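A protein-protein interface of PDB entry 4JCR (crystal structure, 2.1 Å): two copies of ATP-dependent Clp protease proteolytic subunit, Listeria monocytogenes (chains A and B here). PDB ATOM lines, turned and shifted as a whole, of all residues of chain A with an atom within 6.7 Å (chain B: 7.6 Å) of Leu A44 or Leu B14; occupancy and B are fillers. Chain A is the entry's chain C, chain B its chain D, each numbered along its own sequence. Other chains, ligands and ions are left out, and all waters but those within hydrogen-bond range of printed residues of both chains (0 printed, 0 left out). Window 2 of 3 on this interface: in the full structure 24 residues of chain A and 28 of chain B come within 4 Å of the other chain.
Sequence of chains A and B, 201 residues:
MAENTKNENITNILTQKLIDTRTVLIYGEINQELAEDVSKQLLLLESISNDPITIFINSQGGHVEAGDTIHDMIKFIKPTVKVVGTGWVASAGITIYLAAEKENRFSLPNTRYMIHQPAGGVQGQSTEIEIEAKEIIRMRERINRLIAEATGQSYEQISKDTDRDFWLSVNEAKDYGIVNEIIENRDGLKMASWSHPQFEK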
ATOM      1  N   ILE A  19       5.570 -19.487  31.034  1.00  0.00           N
ATOM      2  CA  ILE A  19       6.366 -18.675  30.109  1.00  0.00           C
ATOM      3  C   ILE A  19       5.644 -17.368  29.779  1.00  0.00           C
ATOM      4  O   ILE A  19       6.281 -16.326  29.595  1.00  0.00           O
ATOM      5  CB  ILE A  19       6.712 -19.472  28.827  1.00  0.00           C
ATOM      6  CG1 ILE A  19       7.903 -20.398  29.091  1.00  0.00           C
ATOM      7  CG2 ILE A  19       7.024 -18.547  27.657  1.00  0.00           C
ATOM      8  CD1 ILE A  19       7.947 -21.626  28.207  1.00  0.00           C
ATOM      9  N   ARG A  22       6.227 -14.207  31.989  1.00  0.00           N
ATOM     10  CA  ARG A  22       7.512 -13.506  31.833  1.00  0.00           C
ATOM     11  C   ARG A  22       8.257 -13.390  33.167  1.00  0.00           C
ATOM     12  O   ARG A  22       8.787 -12.329  33.501  1.00  0.00           O
ATOM     13  CB  ARG A  22       7.323 -12.100  31.228  1.00  0.00           C
ATOM     14  CG  ARG A  22       6.268 -11.956  30.137  1.00  0.00           C
ATOM     15  CD  ARG A  22       6.818 -12.214  28.745  1.00  0.00           C
ATOM     16  NE  ARG A  22       7.917 -11.323  28.368  1.00  0.00           N
ATOM     17  CZ  ARG A  22       8.750 -11.560  27.358  1.00  0.00           C
ATOM     18  NH1 ARG A  22       9.724 -10.705  27.079  1.00  0.00           N
ATOM     19  NH2 ARG A  22       8.613 -12.659  26.622  1.00  0.00           N
ATOM     20  N   SER A  39      20.319 -17.452  31.901  1.00  0.00           N
ATOM     21  CA  SER A  39      20.629 -16.965  30.555  1.00  0.00           C
ATOM     22  C   SER A  39      19.697 -17.547  29.501  1.00  0.00           C
ATOM     23  O   SER A  39      19.213 -16.820  28.633  1.00  0.00           O
ATOM     24  CB  SER A  39      22.082 -17.262  30.177  1.00  0.00           C
ATOM     25  OG  SER A  39      22.974 -16.456  30.919  1.00  0.00           O
ATOM     26  N   LYS A  40      19.449 -18.853  29.586  1.00  0.00           N
ATOM     27  CA  LYS A  40      18.555 -19.529  28.646  1.00  0.00           C
ATOM     28  C   LYS A  40      17.130 -19.001  28.756  1.00  0.00           C
ATOM     29  O   LYS A  40      16.474 -18.779  27.736  1.00  0.00           O
ATOM     30  CB  LYS A  40      18.572 -21.045  28.855  1.00  0.00           C
ATOM     31  CG  LYS A  40      19.764 -21.752  28.230  1.00  0.00           C
ATOM     32  CD  LYS A  40      19.752 -23.238  28.560  1.00  0.00           C
ATOM     33  CE  LYS A  40      21.020 -23.925  28.077  1.00  0.00           C
ATOM     34  NZ  LYS A  40      20.991 -25.388  28.366  1.00  0.00           N
ATOM     35  N   GLN A  41      16.664 -18.799  29.990  1.00  0.00           N
ATOM     36  CA  GLN A  41      15.324 -18.264  30.240  1.00  0.00           C
ATOM     37  C   GLN A  41      15.158 -16.849  29.686  1.00  0.00           C
ATOM     38  O   GLN A  41      14.141 -16.546  29.064  1.00  0.00           O
ATOM     39  CB  GLN A  41      14.984 -18.290  31.734  1.00  0.00           C
ATOM     40  CG  GLN A  41      14.794 -19.683  32.315  1.00  0.00           C
ATOM     41  CD  GLN A  41      14.395 -19.654  33.778  1.00  0.00           C
ATOM     42  OE1 GLN A  41      13.377 -19.068  34.143  1.00  0.00           O
ATOM     43  NE2 GLN A  41      15.195 -20.290  34.624  1.00  0.00           N
ATOM     44  N   LEU A  42      16.161 -16.000  29.904  1.00  0.00           N
ATOM     45  CA  LEU A  42      16.136 -14.619  29.411  1.00  0.00           C
ATOM     46  C   LEU A  42      16.218 -14.528  27.885  1.00  0.00           C
ATOM     47  O   LEU A  42      15.511 -13.726  27.271  1.00  0.00           O
ATOM     48  CB  LEU A  42      17.254 -13.783  30.048  1.00  0.00           C
ATOM     49  CG  LEU A  42      17.224 -13.547  31.564  1.00  0.00           C
ATOM     50  CD1 LEU A  42      18.505 -12.850  32.002  1.00  0.00           C
ATOM     51  CD2 LEU A  42      15.998 -12.753  31.994  1.00  0.00           C
ATOM     52  N   LEU A  43      17.081 -15.338  27.278  1.00  0.00           N
ATOM     53  CA  LEU A  43      17.198 -15.378  25.820  1.00  0.00           C
ATOM     54  C   LEU A  43      15.921 -15.908  25.169  1.00  0.00           C
ATOM     55  O   LEU A  43      15.522 -15.434  24.105  1.00  0.00           O
ATOM     56  CB  LEU A  43      18.414 -16.202  25.385  1.00  0.00           C
ATOM     57  CG  LEU A  43      19.789 -15.576  25.644  1.00  0.00           C
ATOM     58  CD1 LEU A  43      20.884 -16.628  25.552  1.00  0.00           C
ATOM     59  CD2 LEU A  43      20.068 -14.416  24.694  1.00  0.00           C
ATOM     60  N   LEU A  44      15.278 -16.873  25.825  1.00  0.00           N
ATOM     61  CA  LEU A  44      14.008 -17.423  25.357  1.00  0.00           C
ATOM     62  C   LEU A  44      12.888 -16.380  25.380  1.00  0.00           C
ATOM     63  O   LEU A  44      12.159 -16.232  24.401  1.00  0.00           O
ATOM     64  CB  LEU A  44      13.602 -18.642  26.192  1.00  0.00           C
ATOM     65  CG  LEU A  44      12.287 -19.334  25.818  1.00  0.00           C
ATOM     66  CD1 LEU A  44      12.536 -20.466  24.834  1.00  0.00           C
ATOM     67  CD2 LEU A  44      11.590 -19.862  27.062  1.00  0.00           C
ATOM     68  N   LEU A  45      12.751 -15.673  26.502  1.00  0.00           N
ATOM     69  CA  LEU A  45      11.706 -14.660  26.648  1.00  0.00           C
ATOM     70  C   LEU A  45      11.907 -13.492  25.683  1.00  0.00           C
ATOM     71  O   LEU A  45      10.936 -12.963  25.140  1.00  0.00           O
ATOM     72  CB  LEU A  45      11.617 -14.159  28.093  1.00  0.00           C
ATOM     73  CG  LEU A  45      11.101 -15.123  29.167  1.00  0.00           C
ATOM     74  CD1 LEU A  45      11.367 -14.545  30.548  1.00  0.00           C
ATOM     75  CD2 LEU A  45       9.621 -15.438  28.996  1.00  0.00           C
ATOM     76  N   GLU A  46      13.167 -13.111  25.469  1.00  0.00           N
ATOM     77  CA  GLU A  46      13.525 -12.082  24.490  1.00  0.00           C
ATOM     78  C   GLU A  46      13.129 -12.471  23.059  1.00  0.00           C
ATOM     79  O   GLU A  46      12.709 -11.618  22.275  1.00  0.00           O
ATOM     80  CB  GLU A  46      15.025 -11.769  24.551  1.00  0.00           C
ATOM     81  CG  GLU A  46      15.500 -10.810  23.466  1.00  0.00           C
ATOM     82  CD  GLU A  46      16.993 -10.551  23.498  1.00  0.00           C
ATOM     83  OE1 GLU A  46      17.779 -11.511  23.666  1.00  0.00           O
ATOM     84  OE2 GLU A  46      17.378  -9.374  23.342  1.00  0.00           O
ATOM     85  N   SER A  47      13.268 -13.754  22.728  1.00  0.00           N
ATOM     86  CA  SER A  47      12.937 -14.250  21.393  1.00  0.00           C
ATOM     87  C   SER A  47      11.431 -14.262  21.144  1.00  0.00           C
ATOM     88  O   SER A  47      10.985 -14.170  19.999  1.00  0.00           O
ATOM     89  CB  SER A  47      13.512 -15.651  21.175  1.00  0.00           C
ATOM     90  OG  SER A  47      12.725 -16.635  21.824  1.00  0.00           O
ATOM     91  N   ILE A  48      10.659 -14.383  22.220  1.00  0.00           N
ATOM     92  CA  ILE A  48       9.201 -14.425  22.137  1.00  0.00           C
ATOM     93  C   ILE A  48       8.621 -13.030  21.893  1.00  0.00           C
ATOM     94  O   ILE A  48       7.865 -12.836  20.942  1.00  0.00           O
ATOM     95  CB  ILE A  48       8.578 -15.106  23.381  1.00  0.00           C
ATOM     96  CG1 ILE A  48       8.937 -16.598  23.393  1.00  0.00           C
ATOM     97  CG2 ILE A  48       7.063 -14.928  23.413  1.00  0.00           C
ATOM     98  CD1 ILE A  48       8.734 -17.286  24.726  1.00  0.00           C
ATOM     99  N   SER A  49       8.992 -12.067  22.738  1.00  0.00           N
ATOM    100  CA  SER A  49       8.530 -10.684  22.602  1.00  0.00           C
ATOM    101  C   SER A  49       9.462  -9.695  23.305  1.00  0.00           C
ATOM    102  O   SER A  49      10.438 -10.095  23.945  1.00  0.00           O
ATOM    103  CB  SER A  49       7.106 -10.533  23.148  1.00  0.00           C
ATOM    104  OG  SER A  49       7.081 -10.663  24.558  1.00  0.00           O
ATOM    105  N   ILE B  13       8.275 -27.476  22.115  1.00  0.00           N
ATOM    106  CA  ILE B  13       8.287 -26.036  21.713  1.00  0.00           C
ATOM    107  C   ILE B  13       9.214 -25.217  22.626  1.00  0.00           C
ATOM    108  O   ILE B  13       9.481 -24.040  22.359  1.00  0.00           O
ATOM    109  CB  ILE B  13       6.860 -25.427  21.699  1.00  0.00           C
ATOM    110  CG1 ILE B  13       5.820 -26.477  21.284  1.00  0.00           C
ATOM    111  CG2 ILE B  13       6.799 -24.217  20.771  1.00  0.00           C
ATOM    112  CD1 ILE B  13       4.413 -26.191  21.768  1.00  0.00           C
ATOM    113  N   LEU B  14       9.711 -25.852  23.689  1.00  0.00           N
ATOM    114  CA  LEU B  14      10.584 -25.190  24.670  1.00  0.00           C
ATOM    115  C   LEU B  14      11.956 -24.812  24.097  1.00  0.00           C
ATOM    116  O   LEU B  14      12.376 -23.658  24.194  1.00  0.00           O
ATOM    117  CB  LEU B  14      10.725 -26.023  25.962  1.00  0.00           C
ATOM    118  CG  LEU B  14      11.344 -27.429  25.969  1.00  0.00           C
ATOM    119  CD1 LEU B  14      12.052 -27.696  27.292  1.00  0.00           C
ATOM    120  CD2 LEU B  14      10.309 -28.509  25.686  1.00  0.00           C
ATOM    121  N   THR B  15      12.641 -25.786  23.502  1.00  0.00           N
ATOM    122  CA  THR B  15      13.959 -25.563  22.909  1.00  0.00           C
ATOM    123  C   THR B  15      13.825 -25.229  21.420  1.00  0.00           C
ATOM    124  O   THR B  15      14.782 -24.773  20.796  1.00  0.00           O
ATOM    125  CB  THR B  15      14.892 -26.778  23.109  1.00  0.00           C
ATOM    126  OG1 THR B  15      14.626 -27.388  24.380  1.00  0.00           O
ATOM    127  CG2 THR B  15      16.360 -26.355  23.053  1.00  0.00           C
ATOM    128  N   GLN B  16      12.630 -25.450  20.870  1.00  0.00           N
ATOM    129  CA  GLN B  16      12.315 -25.131  19.472  1.00  0.00           C
ATOM    130  C   GLN B  16      12.591 -23.662  19.137  1.00  0.00           C
ATOM    131  O   GLN B  16      13.222 -23.361  18.120  1.00  0.00           O
ATOM    132  CB  GLN B  16      10.858 -25.509  19.153  1.00  0.00           C
ATOM    133  CG  GLN B  16      10.234 -24.819  17.942  1.00  0.00           C
ATOM    134  CD  GLN B  16      10.843 -25.245  16.617  1.00  0.00           C
ATOM    135  OE1 GLN B  16      11.066 -26.432  16.370  1.00  0.00           O
ATOM    136  NE2 GLN B  16      11.105 -24.273  15.750  1.00  0.00           N
ATOM    137  N   LYS B  17      12.121 -22.759  19.997  1.00  0.00           N
ATOM    138  CA  LYS B  17      12.365 -21.330  19.815  1.00  0.00           C
ATOM    139  C   LYS B  17      13.766 -20.931  20.289  1.00  0.00           C
ATOM    140  O   LYS B  17      14.306 -19.913  19.848  1.00  0.00           O
ATOM    141  CB  LYS B  17      11.280 -20.492  20.504  1.00  0.00           C
ATOM    142  CG  LYS B  17      11.156 -19.081  19.950  1.00  0.00           C
ATOM    143  CD  LYS B  17       9.764 -18.508  20.149  1.00  0.00           C
ATOM    144  CE  LYS B  17       9.594 -17.220  19.357  1.00  0.00           C
ATOM    145  NZ  LYS B  17       8.199 -16.707  19.414  1.00  0.00           N
ATOM    146  N   LEU B  18      14.350 -21.737  21.177  1.00  0.00           N
ATOM    147  CA  LEU B  18      15.731 -21.531  21.618  1.00  0.00           C
ATOM    148  C   LEU B  18      16.723 -21.911  20.516  1.00  0.00           C
ATOM    149  O   LEU B  18      17.774 -21.288  20.384  1.00  0.00           O
ATOM    150  CB  LEU B  18      16.024 -22.313  22.902  1.00  0.00           C
ATOM    151  CG  LEU B  18      17.264 -21.893  23.705  1.00  0.00           C
ATOM    152  CD1 LEU B  18      17.033 -20.587  24.456  1.00  0.00           C
ATOM    153  CD2 LEU B  18      17.677 -22.995  24.669  1.00  0.00           C
ATOM    154  N   ILE B  19      16.375 -22.933  19.733  1.00  0.00           N
ATOM    155  CA  ILE B  19      17.158 -23.352  18.566  1.00  0.00           C
ATOM    156  C   ILE B  19      17.111 -22.284  17.467  1.00  0.00           C
ATOM    157  O   ILE B  19      18.091 -22.087  16.745  1.00  0.00           O
ATOM    158  CB  ILE B  19      16.692 -24.736  18.044  1.00  0.00           C
ATOM    159  CG1 ILE B  19      17.222 -25.847  18.960  1.00  0.00           C
ATOM    160  CG2 ILE B  19      17.155 -24.987  16.616  1.00  0.00           C
ATOM    161  CD1 ILE B  19      16.438 -27.143  18.900  1.00  0.00           C
ATOM    162  N   THR B  21      17.129 -19.129  17.986  1.00  0.00           N
ATOM    163  CA  THR B  21      18.045 -18.056  18.389  1.00  0.00           C
ATOM    164  C   THR B  21      19.490 -18.311  17.949  1.00  0.00           C
ATOM    165  O   THR B  21      20.307 -17.392  17.944  1.00  0.00           O
ATOM    166  CB  THR B  21      18.026 -17.808  19.915  1.00  0.00           C
ATOM    167  OG1 THR B  21      18.551 -18.951  20.602  1.00  0.00           O
ATOM    168  CG2 THR B  21      16.615 -17.521  20.404  1.00  0.00           C
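The side-chain hydroxyl (OG) of Ser A47 sits at hydrogen-bond distance from the backbone carbonyl oxygen (O) of Leu A44 (2.7 Å). The side-chain hydroxyl (OG1) of Thr B21 lies within hydrogen-bond range of the backbone carbonyl oxygen (O) of Leu B18 (2.5 Å).
Lys A40 touches Leu B18 (O to CD1, 3.8 Å). Leu A44 touches Leu B14 (CD1 to O, 3.3 Å). CE of Lys B17 touches O of Ser A47, at 3.4 Å. Thr B21 touches Ser A47. Lys B17 touches Ile A48.
Leu A44 touches just one residue of chain B: Leu B14 (3.3 Å). Of the printed residues of chain B, Ser A47 touches Lys B17 and Thr B21. Of the printed residues of chain B, Ile A48 touches Lys B17. Leu B14 touches one residue of chain A. Of the printed residues of chain A, Lys B17 touches Ser A47 (3.4 Å) and Ile A48 (3.7 Å). Of the printed residues of chain A, Leu B18 touches Lys A40 (3.8 Å). Printed residues of chain A within 4 Å of Thr B21: Ser A47.
Printed residues of chain A that touch a printed residue of chain B: Lys A40, Leu A44, Ser A47 and Ile A48. Hydrophobic or aromatic side chains of chain A that line the printed part of chain B: Leu A44 and Ile A48.
Position printed for both chains: 19. Of the 5 pairs that touch across the chains among the printed residues, none has its exchanged pair printed and touching as well.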
